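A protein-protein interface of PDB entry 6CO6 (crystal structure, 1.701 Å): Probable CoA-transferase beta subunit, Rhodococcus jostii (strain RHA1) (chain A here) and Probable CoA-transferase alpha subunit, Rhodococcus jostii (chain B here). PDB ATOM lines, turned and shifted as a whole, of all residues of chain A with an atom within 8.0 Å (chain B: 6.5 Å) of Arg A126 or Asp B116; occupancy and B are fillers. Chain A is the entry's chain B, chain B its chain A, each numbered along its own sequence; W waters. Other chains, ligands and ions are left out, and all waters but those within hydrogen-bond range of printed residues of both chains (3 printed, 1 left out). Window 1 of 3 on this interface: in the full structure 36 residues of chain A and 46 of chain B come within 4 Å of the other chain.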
ATOM      1  N   MET A  33      11.483  16.410 -18.480  1.00  0.00           N
ATOM      2  CA  MET A  33      11.899  17.381 -19.485  1.00  0.00           C
ATOM      3  C   MET A  33      12.722  16.762 -20.602  1.00  0.00           C
ATOM      4  O   MET A  33      13.438  17.483 -21.299  1.00  0.00           O
ATOM      5  CB  MET A  33      12.685  18.524 -18.841  1.00  0.00           C
ATOM      6  CG  MET A  33      11.981  19.179 -17.681  1.00  0.00           C
ATOM      7  SD  MET A  33      10.386  19.865 -18.143  1.00  0.00           S
ATOM      8  CE  MET A  33      10.872  21.098 -19.334  1.00  0.00           C
ATOM      9  N   PHE A  84       4.144  27.995 -11.987  1.00  0.00           N
ATOM     10  CA  PHE A  84       4.944  28.592 -10.926  1.00  0.00           C
ATOM     11  C   PHE A  84       4.248  28.493  -9.572  1.00  0.00           C
ATOM     12  O   PHE A  84       4.923  28.373  -8.544  1.00  0.00           O
ATOM     13  CB  PHE A  84       5.277  30.033 -11.295  1.00  0.00           C
ATOM     14  CG  PHE A  84       6.069  30.143 -12.568  1.00  0.00           C
ATOM     15  CD1 PHE A  84       7.161  29.320 -12.780  1.00  0.00           C
ATOM     16  CD2 PHE A  84       5.711  31.039 -13.552  1.00  0.00           C
ATOM     17  CE1 PHE A  84       7.891  29.401 -13.952  1.00  0.00           C
ATOM     18  CE2 PHE A  84       6.449  31.129 -14.725  1.00  0.00           C
ATOM     19  CZ  PHE A  84       7.523  30.300 -14.922  1.00  0.00           C
ATOM     20  N   VAL A  87       5.070  24.957  -8.521  1.00  0.00           N
ATOM     21  CA  VAL A  87       6.447  24.896  -8.026  1.00  0.00           C
ATOM     22  C   VAL A  87       6.507  25.376  -6.585  1.00  0.00           C
ATOM     23  O   VAL A  87       7.066  24.707  -5.712  1.00  0.00           O
ATOM     24  CB  VAL A  87       7.394  25.723  -8.915  1.00  0.00           C
ATOM     25  CG1 VAL A  87       8.766  25.851  -8.250  1.00  0.00           C
ATOM     26  CG2 VAL A  87       7.527  25.087 -10.302  1.00  0.00           C
ATOM     27  N   MET A  96      15.035  17.104 -14.876  1.00  0.00           N
ATOM     28  CA  MET A  96      15.714  18.011 -15.793  1.00  0.00           C
ATOM     29  C   MET A  96      16.901  17.322 -16.452  1.00  0.00           C
ATOM     30  O   MET A  96      17.429  16.324 -15.953  1.00  0.00           O
ATOM     31  CB  MET A  96      16.205  19.267 -15.056  1.00  0.00           C
ATOM     32  CG  MET A  96      15.077  20.107 -14.450  1.00  0.00           C
ATOM     33  SD  MET A  96      15.677  21.668 -13.773  1.00  0.00           S
ATOM     34  CE  MET A  96      16.329  21.160 -12.184  1.00  0.00           C
ATOM     35  N   GLY A  97      17.307  17.863 -17.602  1.00  0.00           N
ATOM     36  CA  GLY A  97      18.597  17.539 -18.164  1.00  0.00           C
ATOM     37  C   GLY A  97      19.683  18.312 -17.437  1.00  0.00           C
ATOM     38  O   GLY A  97      19.434  19.080 -16.509  1.00  0.00           O
ATOM     39  N   LEU A 109      22.627  24.074 -16.433  1.00  0.00           N
ATOM     40  CA  LEU A 109      22.116  24.065 -17.804  1.00  0.00           C
ATOM     41  C   LEU A 109      22.074  25.470 -18.400  1.00  0.00           C
ATOM     42  O   LEU A 109      21.436  25.673 -19.439  1.00  0.00           O
ATOM     43  CB  LEU A 109      20.728  23.413 -17.872  1.00  0.00           C
ATOM     44  CG  LEU A 109      19.674  23.806 -16.829  1.00  0.00           C
ATOM     45  CD1 LEU A 109      19.304  25.288 -16.906  1.00  0.00           C
ATOM     46  CD2 LEU A 109      18.433  22.930 -17.003  1.00  0.00           C
ATOM     47  N   SER A 110      22.754  26.438 -17.788  1.00  0.00           N
ATOM     48  CA  SER A 110      22.640  27.835 -18.204  1.00  0.00           C
ATOM     49  C   SER A 110      23.582  28.174 -19.355  1.00  0.00           C
ATOM     50  O   SER A 110      23.138  28.590 -20.432  1.00  0.00           O
ATOM     51  CB  SER A 110      22.918  28.759 -17.014  1.00  0.00           C
ATOM     52  OG  SER A 110      23.033  30.102 -17.435  1.00  0.00           O
ATOM     53  N   MET A 122      23.581  28.532 -23.471  1.00  0.00           N
ATOM     54  CA  MET A 122      22.405  27.687 -23.656  1.00  0.00           C
ATOM     55  C   MET A 122      21.155  28.499 -23.321  1.00  0.00           C
ATOM     56  O   MET A 122      21.094  29.679 -23.674  1.00  0.00           O
ATOM     57  CB  MET A 122      22.521  26.400 -22.838  1.00  0.00           C
ATOM     58  CG  MET A 122      23.589  25.464 -23.415  1.00  0.00           C
ATOM     59  SD  MET A 122      25.230  25.817 -22.763  1.00  0.00           S
ATOM     60  CE  MET A 122      25.050  25.122 -21.113  1.00  0.00           C
ATOM     61  N   PHE A 123      20.147  27.906 -22.671  1.00  0.00           N
ATOM     62  CA  PHE A 123      18.908  28.659 -22.464  1.00  0.00           C
ATOM     63  C   PHE A 123      18.953  29.618 -21.278  1.00  0.00           C
ATOM     64  O   PHE A 123      18.029  30.429 -21.136  1.00  0.00           O
ATOM     65  CB  PHE A 123      17.704  27.718 -22.250  1.00  0.00           C
ATOM     66  CG  PHE A 123      17.355  26.872 -23.437  1.00  0.00           C
ATOM     67  CD1 PHE A 123      17.133  27.441 -24.682  1.00  0.00           C
ATOM     68  CD2 PHE A 123      17.221  25.499 -23.300  1.00  0.00           C
ATOM     69  CE1 PHE A 123      16.802  26.654 -25.775  1.00  0.00           C
ATOM     70  CE2 PHE A 123      16.885  24.707 -24.383  1.00  0.00           C
ATOM     71  CZ  PHE A 123      16.680  25.284 -25.625  1.00  0.00           C
ATOM     72  N   GLY A 124      19.977  29.557 -20.426  1.00  0.00           N
ATOM     73  CA  GLY A 124      19.919  30.227 -19.136  1.00  0.00           C
ATOM     74  C   GLY A 124      19.357  29.306 -18.065  1.00  0.00           C
ATOM     75  O   GLY A 124      19.037  28.143 -18.316  1.00  0.00           O
ATOM     76  N   VAL A 125      19.205  29.843 -16.842  1.00  0.00           N
ATOM     77  CA  VAL A 125      18.873  28.977 -15.701  1.00  0.00           C
ATOM     78  C   VAL A 125      17.460  28.394 -15.770  1.00  0.00           C
ATOM     79  O   VAL A 125      17.178  27.407 -15.074  1.00  0.00           O
ATOM     80  CB  VAL A 125      19.045  29.691 -14.341  1.00  0.00           C
ATOM     81  CG1 VAL A 125      20.514  30.042 -14.096  1.00  0.00           C
ATOM     82  CG2 VAL A 125      18.128  30.927 -14.226  1.00  0.00           C
ATOM     83  N   ARG A 126      16.563  28.973 -16.572  1.00  0.00           N
ATOM     84  CA  ARG A 126      15.177  28.481 -16.723  1.00  0.00           C
ATOM     85  C   ARG A 126      14.533  28.377 -15.341  1.00  0.00           C
ATOM     86  O   ARG A 126      14.597  29.334 -14.555  1.00  0.00           O
ATOM     87  CB  ARG A 126      15.173  27.178 -17.519  1.00  0.00           C
ATOM     88  CG  ARG A 126      15.719  27.299 -18.937  1.00  0.00           C
ATOM     89  CD  ARG A 126      15.779  25.932 -19.588  1.00  0.00           C
ATOM     90  NE  ARG A 126      14.465  25.464 -20.019  1.00  0.00           N
ATOM     91  CZ  ARG A 126      14.247  24.313 -20.655  1.00  0.00           C
ATOM     92  NH1 ARG A 126      15.251  23.492 -20.924  1.00  0.00           N
ATOM     93  NH2 ARG A 126      13.014  23.979 -21.014  1.00  0.00           N
ATOM     94  N   GLY A 127      13.896  27.262 -15.005  1.00  0.00           N
ATOM     95  CA  GLY A 127      13.314  27.056 -13.698  1.00  0.00           C
ATOM     96  C   GLY A 127      14.170  26.251 -12.750  1.00  0.00           C
ATOM     97  O   GLY A 127      13.695  25.890 -11.671  1.00  0.00           O
ATOM     98  N   ALA A 128      15.419  25.957 -13.113  1.00  0.00           N
ATOM     99  CA  ALA A 128      16.240  25.103 -12.259  1.00  0.00           C
ATOM    100  C   ALA A 128      16.412  25.653 -10.845  1.00  0.00           C
ATOM    101  O   ALA A 128      16.361  24.847  -9.900  1.00  0.00           O
ATOM    102  CB  ALA A 128      17.599  24.850 -12.932  1.00  0.00           C
ATOM    103  N   PRO A 129      16.639  26.957 -10.617  1.00  0.00           N
ATOM    104  CA  PRO A 129      16.783  27.414  -9.219  1.00  0.00           C
ATOM    105  C   PRO A 129      15.510  27.242  -8.407  1.00  0.00           C
ATOM    106  O   PRO A 129      15.557  26.728  -7.277  1.00  0.00           O
ATOM    107  CB  PRO A 129      17.184  28.892  -9.369  1.00  0.00           C
ATOM    108  CG  PRO A 129      17.821  28.979 -10.772  1.00  0.00           C
ATOM    109  CD  PRO A 129      16.953  28.042 -11.576  1.00  0.00           C
ATOM    110  N   GLY A 130      14.361  27.643  -8.960  1.00  0.00           N
ATOM    111  CA  GLY A 130      13.108  27.455  -8.244  1.00  0.00           C
ATOM    112  C   GLY A 130      12.742  25.994  -8.058  1.00  0.00           C
ATOM    113  O   GLY A 130      12.193  25.612  -7.021  1.00  0.00           O
ATOM    114  N   ASN A 131      13.028  25.159  -9.060  1.00  0.00           N
ATOM    115  CA  ASN A 131      12.720  23.734  -8.938  1.00  0.00           C
ATOM    116  C   ASN A 131      13.501  23.113  -7.793  1.00  0.00           C
ATOM    117  O   ASN A 131      12.924  22.462  -6.913  1.00  0.00           O
ATOM    118  CB  ASN A 131      13.046  22.981 -10.234  1.00  0.00           C
ATOM    119  CG  ASN A 131      12.183  23.418 -11.408  1.00  0.00           C
ATOM    120  OD1 ASN A 131      11.165  24.092 -11.232  1.00  0.00           O
ATOM    121  ND2 ASN A 131      12.583  23.026 -12.619  1.00  0.00           N
ATOM    122  N   THR A 132      14.817  23.320  -7.788  1.00  0.00           N
ATOM    123  CA  THR A 132      15.675  22.650  -6.822  1.00  0.00           C
ATOM    124  C   THR A 132      15.490  23.180  -5.408  1.00  0.00           C
ATOM    125  O   THR A 132      15.749  22.442  -4.454  1.00  0.00           O
ATOM    126  CB  THR A 132      17.145  22.763  -7.238  1.00  0.00           C
ATOM    127  OG1 THR A 132      17.475  24.132  -7.520  1.00  0.00           O
ATOM    128  CG2 THR A 132      17.408  21.887  -8.469  1.00  0.00           C
ATOM    129  N   ILE A 133      15.030  24.421  -5.238  1.00  0.00           N
ATOM    130  CA  ILE A 133      14.793  24.908  -3.884  1.00  0.00           C
ATOM    131  C   ILE A 133      13.404  24.532  -3.371  1.00  0.00           C
ATOM    132  O   ILE A 133      13.179  24.568  -2.154  1.00  0.00           O
ATOM    133  CB  ILE A 133      15.020  26.434  -3.791  1.00  0.00           C
ATOM    134  CG1 ILE A 133      15.300  26.866  -2.344  1.00  0.00           C
ATOM    135  CG2 ILE A 133      13.836  27.216  -4.365  1.00  0.00           C
ATOM    136  CD1 ILE A 133      16.603  26.354  -1.769  1.00  0.00           C
ATOM    137  N   ASN A 134      12.479  24.134  -4.246  1.00  0.00           N
ATOM    138  CA  ASN A 134      11.095  23.935  -3.811  1.00  0.00           C
ATOM    139  C   ASN A 134      10.635  22.487  -3.713  1.00  0.00           C
ATOM    140  O   ASN A 134       9.743  22.213  -2.912  1.00  0.00           O
ATOM    141  CB  ASN A 134      10.126  24.662  -4.752  1.00  0.00           C
ATOM    142  CG  ASN A 134       9.901  26.097  -4.351  1.00  0.00           C
ATOM    143  OD1 ASN A 134       9.311  26.379  -3.297  1.00  0.00           O
ATOM    144  ND2 ASN A 134      10.376  27.019  -5.176  1.00  0.00           N
ATOM    145  N   SER A 157      22.907  26.516 -11.745  1.00  0.00           N
ATOM    146  CA  SER A 157      21.488  26.723 -12.008  1.00  0.00           C
ATOM    147  C   SER A 157      20.611  25.837 -11.124  1.00  0.00           C
ATOM    148  O   SER A 157      19.537  26.276 -10.703  1.00  0.00           O
ATOM    149  CB  SER A 157      21.174  26.491 -13.499  1.00  0.00           C
ATOM    150  OG  SER A 157      21.559  25.195 -13.930  1.00  0.00           O
ATOM    151  N   TYR B  67      10.692  37.025 -21.000  1.00  0.00           N
ATOM    152  CA  TYR B  67      10.890  35.592 -21.192  1.00  0.00           C
ATOM    153  C   TYR B  67      11.373  35.469 -22.631  1.00  0.00           C
ATOM    154  O   TYR B  67      10.577  35.470 -23.573  1.00  0.00           O
ATOM    155  CB  TYR B  67       9.599  34.819 -20.936  1.00  0.00           C
ATOM    156  CG  TYR B  67       9.186  34.738 -19.479  1.00  0.00           C
ATOM    157  CD1 TYR B  67       9.966  34.055 -18.546  1.00  0.00           C
ATOM    158  CD2 TYR B  67       7.983  35.304 -19.037  1.00  0.00           C
ATOM    159  CE1 TYR B  67       9.564  33.945 -17.206  1.00  0.00           C
ATOM    160  CE2 TYR B  67       7.587  35.210 -17.702  1.00  0.00           C
ATOM    161  CZ  TYR B  67       8.383  34.534 -16.796  1.00  0.00           C
ATOM    162  OH  TYR B  67       7.975  34.414 -15.487  1.00  0.00           O
ATOM    163  N   TYR B  86      15.959  38.289 -17.504  1.00  0.00           N
ATOM    164  CA  TYR B  86      15.226  37.226 -18.187  1.00  0.00           C
ATOM    165  C   TYR B  86      15.298  35.945 -17.375  1.00  0.00           C
ATOM    166  O   TYR B  86      16.223  35.736 -16.589  1.00  0.00           O
ATOM    167  CB  TYR B  86      15.779  36.988 -19.603  1.00  0.00           C
ATOM    168  CG  TYR B  86      17.256  36.667 -19.592  1.00  0.00           C
ATOM    169  CD1 TYR B  86      17.699  35.358 -19.469  1.00  0.00           C
ATOM    170  CD2 TYR B  86      18.208  37.681 -19.664  1.00  0.00           C
ATOM    171  CE1 TYR B  86      19.050  35.063 -19.430  1.00  0.00           C
ATOM    172  CE2 TYR B  86      19.571  37.394 -19.629  1.00  0.00           C
ATOM    173  CZ  TYR B  86      19.976  36.082 -19.509  1.00  0.00           C
ATOM    174  OH  TYR B  86      21.316  35.787 -19.468  1.00  0.00           O
ATOM    175  N   GLY B  87      14.323  35.070 -17.610  1.00  0.00           N
ATOM    176  CA  GLY B  87      14.344  33.754 -16.997  1.00  0.00           C
ATOM    177  C   GLY B  87      14.949  32.709 -17.917  1.00  0.00           C
ATOM    178  O   GLY B  87      15.441  31.671 -17.471  1.00  0.00           O
ATOM    179  N   PHE B  88      14.893  32.976 -19.214  1.00  0.00           N
ATOM    180  CA  PHE B  88      15.509  32.120 -20.221  1.00  0.00           C
ATOM    181  C   PHE B  88      15.530  32.916 -21.516  1.00  0.00           C
ATOM    182  O   PHE B  88      14.881  33.957 -21.632  1.00  0.00           O
ATOM    183  CB  PHE B  88      14.714  30.818 -20.411  1.00  0.00           C
ATOM    184  CG  PHE B  88      13.342  31.049 -20.972  1.00  0.00           C
ATOM    185  CD1 PHE B  88      13.137  31.130 -22.348  1.00  0.00           C
ATOM    186  CD2 PHE B  88      12.259  31.218 -20.130  1.00  0.00           C
ATOM    187  CE1 PHE B  88      11.883  31.375 -22.867  1.00  0.00           C
ATOM    188  CE2 PHE B  88      11.002  31.454 -20.650  1.00  0.00           C
ATOM    189  CZ  PHE B  88      10.813  31.533 -22.019  1.00  0.00           C
ATOM    190  N   VAL B  89      16.254  32.391 -22.506  1.00  0.00           N
ATOM    191  CA  VAL B  89      16.112  32.819 -23.892  1.00  0.00           C
ATOM    192  C   VAL B  89      16.019  31.561 -24.735  1.00  0.00           C
ATOM    193  O   VAL B  89      16.923  30.713 -24.694  1.00  0.00           O
ATOM    194  CB  VAL B  89      17.279  33.711 -24.363  1.00  0.00           C
ATOM    195  CG1 VAL B  89      17.062  34.124 -25.804  1.00  0.00           C
ATOM    196  CG2 VAL B  89      17.392  34.951 -23.455  1.00  0.00           C
ATOM    197  N   GLU B 114      20.167  37.509 -15.148  1.00  0.00           N
ATOM    198  CA  GLU B 114      19.465  36.261 -15.387  1.00  0.00           C
ATOM    199  C   GLU B 114      18.895  35.768 -14.056  1.00  0.00           C
ATOM    200  O   GLU B 114      19.478  35.992 -12.990  1.00  0.00           O
ATOM    201  CB  GLU B 114      20.445  35.274 -16.031  1.00  0.00           C
ATOM    202  CG  GLU B 114      20.033  33.822 -16.118  1.00  0.00           C
ATOM    203  CD  GLU B 114      21.003  33.021 -16.989  1.00  0.00           C
ATOM    204  OE1 GLU B 114      21.656  33.596 -17.900  1.00  0.00           O
ATOM    205  OE2 GLU B 114      21.164  31.812 -16.730  1.00  0.00           O
ATOM    206  N   MET B 115      17.721  35.151 -14.108  1.00  0.00           N
ATOM    207  CA  MET B 115      17.031  34.780 -12.883  1.00  0.00           C
ATOM    208  C   MET B 115      16.160  33.570 -13.164  1.00  0.00           C
ATOM    209  O   MET B 115      15.913  33.220 -14.320  1.00  0.00           O
ATOM    210  CB  MET B 115      16.173  35.940 -12.355  1.00  0.00           C
ATOM    211  CG  MET B 115      14.929  36.210 -13.195  1.00  0.00           C
ATOM    212  SD  MET B 115      14.086  37.724 -12.679  1.00  0.00           S
ATOM    213  CE  MET B 115      14.740  38.899 -13.881  1.00  0.00           C
ATOM    214  N   ASP B 116      15.710  32.922 -12.089  1.00  0.00           N
ATOM    215  CA  ASP B 116      14.758  31.829 -12.228  1.00  0.00           C
ATOM    216  C   ASP B 116      13.476  32.332 -12.890  1.00  0.00           C
ATOM    217  O   ASP B 116      13.055  33.467 -12.673  1.00  0.00           O
ATOM    218  CB  ASP B 116      14.448  31.225 -10.855  1.00  0.00           C
ATOM    219  CG  ASP B 116      13.297  30.232 -10.898  1.00  0.00           C
ATOM    220  OD1 ASP B 116      13.534  29.033 -11.164  1.00  0.00           O
ATOM    221  OD2 ASP B 116      12.147  30.648 -10.657  1.00  0.00           O
ATOM    222  N   GLU B 117      12.858  31.472 -13.713  1.00  0.00           N
ATOM    223  CA  GLU B 117      11.643  31.855 -14.435  1.00  0.00           C
ATOM    224  C   GLU B 117      10.558  32.396 -13.511  1.00  0.00           C
ATOM    225  O   GLU B 117       9.856  33.359 -13.858  1.00  0.00           O
ATOM    226  CB  GLU B 117      11.090  30.654 -15.197  1.00  0.00           C
ATOM    227  CG  GLU B 117      11.809  30.354 -16.468  1.00  0.00           C
ATOM    228  CD  GLU B 117      11.460  28.968 -16.977  1.00  0.00           C
ATOM    229  OE1 GLU B 117      10.621  28.282 -16.343  1.00  0.00           O
ATOM    230  OE2 GLU B 117      12.034  28.570 -17.999  1.00  0.00           O
ATOM    231  N   GLY B 118      10.365  31.762 -12.352  1.00  0.00           N
ATOM    232  CA  GLY B 118       9.347  32.231 -11.426  1.00  0.00           C
ATOM    233  C   GLY B 118       9.655  33.599 -10.850  1.00  0.00           C
ATOM    234  O   GLY B 118       8.742  34.324 -10.437  1.00  0.00           O
ATOM    235  N   MET B 119      10.937  33.966 -10.804  1.00  0.00           N
ATOM    236  CA  MET B 119      11.307  35.282 -10.291  1.00  0.00           C
ATOM    237  C   MET B 119      10.859  36.402 -11.225  1.00  0.00           C
ATOM    238  O   MET B 119      10.589  37.511 -10.760  1.00  0.00           O
ATOM    239  CB  MET B 119      12.814  35.353 -10.053  1.00  0.00           C
ATOM    240  CG  MET B 119      13.299  34.345  -9.023  1.00  0.00           C
ATOM    241  SD  MET B 119      15.093  34.288  -8.912  1.00  0.00           S
ATOM    242  CE  MET B 119      15.475  35.874  -8.203  1.00  0.00           C
ATOM    243  N   VAL B 120      10.791  36.148 -12.539  1.00  0.00           N
ATOM    244  CA  VAL B 120      10.286  37.177 -13.448  1.00  0.00           C
ATOM    245  C   VAL B 120       8.838  37.501 -13.115  1.00  0.00           C
ATOM    246  O   VAL B 120       8.468  38.669 -12.954  1.00  0.00           O
ATOM    247  CB  VAL B 120      10.416  36.741 -14.918  1.00  0.00           C
ATOM    248  CG1 VAL B 120       9.833  37.833 -15.815  1.00  0.00           C
ATOM    249  CG2 VAL B 120      11.866  36.451 -15.286  1.00  0.00           C
ATOM    250  N   LYS B 121       7.997  36.466 -13.017  1.00  0.00           N
ATOM    251  CA  LYS B 121       6.592  36.666 -12.670  1.00  0.00           C
ATOM    252  C   LYS B 121       6.472  37.425 -11.356  1.00  0.00           C
ATOM    253  O   LYS B 121       5.707  38.390 -11.240  1.00  0.00           O
ATOM    254  CB  LYS B 121       5.874  35.313 -12.582  1.00  0.00           C
ATOM    255  CG  LYS B 121       4.412  35.414 -12.117  1.00  0.00           C
ATOM    256  CD  LYS B 121       3.825  34.049 -11.744  1.00  0.00           C
ATOM    257  CE  LYS B 121       2.370  34.196 -11.329  1.00  0.00           C
ATOM    258  NZ  LYS B 121       1.763  32.926 -10.857  1.00  0.00           N
ATOM    259  N   ILE B 136      10.531  35.352  -2.107  1.00  0.00           N
ATOM    260  CA  ILE B 136      10.435  34.148  -2.930  1.00  0.00           C
ATOM    261  C   ILE B 136      11.594  33.240  -2.550  1.00  0.00           C
ATOM    262  O   ILE B 136      12.665  33.714  -2.159  1.00  0.00           O
ATOM    263  CB  ILE B 136      10.432  34.511  -4.440  1.00  0.00           C
ATOM    264  CG1 ILE B 136      10.089  33.294  -5.310  1.00  0.00           C
ATOM    265  CG2 ILE B 136      11.772  35.164  -4.870  1.00  0.00           C
ATOM    266  CD1 ILE B 136       9.709  33.638  -6.757  1.00  0.00           C
ATOM    267  N   ALA B 138      12.844  30.836  -4.772  1.00  0.00           N
ATOM    268  CA  ALA B 138      13.653  30.675  -5.975  1.00  0.00           C
ATOM    269  C   ALA B 138      14.796  31.679  -6.002  1.00  0.00           C
ATOM    270  O   ALA B 138      14.599  32.873  -5.763  1.00  0.00           O
ATOM    271  CB  ALA B 138      12.779  30.843  -7.221  1.00  0.00           C
ATOM    272  N   GLY B 139      15.997  31.178  -6.286  1.00  0.00           N
ATOM    273  CA  GLY B 139      17.184  32.009  -6.294  1.00  0.00           C
ATOM    274  C   GLY B 139      18.156  31.644  -5.186  1.00  0.00           C
ATOM    275  O   GLY B 139      19.373  31.694  -5.390  1.00  0.00           O
ATOM    276  N   VAL B 144      22.044  32.588  -9.425  1.00  0.00           N
ATOM    277  CA  VAL B 144      21.264  33.811  -9.576  1.00  0.00           C
ATOM    278  C   VAL B 144      21.829  34.891  -8.655  1.00  0.00           C
ATOM    279  O   VAL B 144      21.878  36.079  -9.015  1.00  0.00           O
ATOM    280  CB  VAL B 144      19.769  33.546  -9.301  1.00  0.00           C
ATOM    281  CG1 VAL B 144      18.972  34.843  -9.393  1.00  0.00           C
ATOM    282  CG2 VAL B 144      19.217  32.549 -10.319  1.00  0.00           C
ATOM    283  N   TRP B 148      23.402  38.761 -10.007  1.00  0.00           N
ATOM    284  CA  TRP B 148      22.855  40.028  -9.528  1.00  0.00           C
ATOM    285  C   TRP B 148      23.756  40.750  -8.539  1.00  0.00           C
ATOM    286  O   TRP B 148      23.705  41.984  -8.459  1.00  0.00           O
ATOM    287  CB  TRP B 148      21.500  39.805  -8.847  1.00  0.00           C
ATOM    288  CG  TRP B 148      20.364  39.442  -9.745  1.00  0.00           C
ATOM    289  CD1 TRP B 148      20.249  38.314 -10.510  1.00  0.00           C
ATOM    290  CD2 TRP B 148      19.146  40.180  -9.926  1.00  0.00           C
ATOM    291  NE1 TRP B 148      19.040  38.315 -11.175  1.00  0.00           N
ATOM    292  CE2 TRP B 148      18.350  39.452 -10.838  1.00  0.00           C
ATOM    293  CE3 TRP B 148      18.656  41.391  -9.412  1.00  0.00           C
ATOM    294  CZ2 TRP B 148      17.088  39.889 -11.242  1.00  0.00           C
ATOM    295  CZ3 TRP B 148      17.407  41.831  -9.824  1.00  0.00           C
ATOM    296  CH2 TRP B 148      16.637  41.082 -10.733  1.00  0.00           C
HETATM  297  O   HOH W   1      23.485  32.125 -19.282  1.00  0.00           O
HETATM  298  O   HOH W   2      10.061  29.818  -5.069  1.00  0.00           O
HETATM  299  O   HOH W   3      17.178  28.676  -5.954  1.00  0.00           O
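N of Arg A126 lies within hydrogen-bond range of O of Gly B87 (3.1 Å). The backbone NH (N) of Val B89 lies within hydrogen-bond range of the backbone carbonyl oxygen (O) of Phe A123, 3.0 Å away. The side-chain hydroxyl of Ser A110 is in hydrogen-bond range of the side-chain carboxylate of Glu B114 (2.6 Å). The backbone NH (N) of Val A125 lies within hydrogen-bond range of the side-chain carboxylate (OE2) of Glu B114, 2.8 Å away. The side-chain carboxylate (OD1) of Asp B116 sits at hydrogen-bond distance from the backbone NH (N) of Gly A130 (2.7 Å). N of Glu B117 sits at hydrogen-bond distance from O of Arg A126. The backbone carbonyl oxygen (O) of Gly A127 sits close to the side-chain carboxylate (OD1) of Asp B116 (3.2 Å).
The backbone NH (N) of Met B115 is in hydrogen-bond range of the backbone carbonyl oxygen (O) of Tyr B86, 3.0 Å away. The backbone NH of Asp B116 is in hydrogen-bond range of the side-chain sulfur of Met B119 (3.5 Å). N of Gly A124 lies within hydrogen-bond range of O of Ser A110 (3.3 Å). The backbone carbonyl oxygen (O) of Gly A127 sits close to the side-chain amide oxygen (OD1) of Asn A131, 3.1 Å away. O of Pro A129 is in hydrogen-bond range of OG1 of Thr A132.
Among the printed residues, merely in contact across the chains: Phe A84 with Tyr B67 (3.7 Å), Phe A84 with Glu B117 (3.6 Å), Phe A84 with Gly B118 (3.8 Å), Phe A84 with Lys B121 (3.99 Å), Phe A123 with Phe B88 (3.2 Å), Gly A124 with Glu B114 (3.1 Å), Val A125 with Met B115 (3.2 Å), Val A125 with Asp B116 (3.8 Å), Arg A126 with Phe B88 (3.9 Å), Arg A126 with Asp B116 (3.4 Å), Gly A127 with Glu B117 (3.6 Å), Pro A129 with Asp B116 (3.6 Å), Pro A129 with Val B144 (3.9 Å), Gly A130 with Ala B138 (3.6 Å) and Ile A133 with Ala B138 (3.8 Å).
Val A87 touches none of the printed residues of chain B. Of chain B, only Gly B87 (3.1 Å), Phe B88 (3.9 Å), Asp B116 (3.4 Å) and Glu B117 (2.9 Å) come within 4 Å of Arg A126. Of the printed residues of chain B, Gly A127 touches Asp B116 (3.2 Å) and Glu B117 (3.6 Å). Of the printed residues of chain A, Tyr B67 touches Phe A84. Tyr B86 touches none of the printed residues of chain A. Of chain A, only Val A125 (3.8 Å), Arg A126 (3.4 Å), Gly A127 (3.2 Å), Pro A129 (3.6 Å) and Gly A130 (2.7 Å) come within 4 Å of Asp B116. Printed residues of chain A within 4 Å of Gly B118: Phe A84 (3.8 Å). Of the printed residues of chain A, Lys B121 touches Phe A84 (3.99 Å). Of the printed residues of chain A, Val B144 touches Pro A129. The nearest residue of chain B that does not touch Arg A126 is Met B115 (4.1 Å).
Printed residues of chain B that touch a printed residue of chain A: Tyr B67, Gly B87, Phe B88, Val B89, Glu B114, Met B115, Asp B116, Glu B117, Gly B118, Lys B121, Ala B138 and Val B144. Hydrophobic or aromatic side chains of chain B within 4 Å of the printed part of chain A: Tyr B67, Phe B88, Ala B138 and Val B144. Printed residues of chain A that touch a printed residue of chain B: Phe A84, Ser A110, Phe A123, Gly A124, Val A125, Arg A126, Gly A127, Pro A129, Gly A130 and Ile A133. Along chain A the printed residues that touch a printed residue of chain B span positions 84 to 133. Among the printed residues, 22 pairs touch across the chains. Among the printed residues, no Asp or Glu carboxylate lies within 4 Å of a Lys or Arg side-chain nitrogen of the other chain.
Water W1 lies within hydrogen-bond range of the side-chain carboxylate (OE1) of Glu B114 (2.7 Å) and the side-chain hydroxyl (OG) of Ser A110 (2.8 Å). Water W3 lies within hydrogen-bond range of N of Gly B139 and O of Pro A129. Water W2 lies within hydrogen-bond range of ND2 of Asn A134 (2.8 Å) and N of Ala B138 (3.0 Å).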
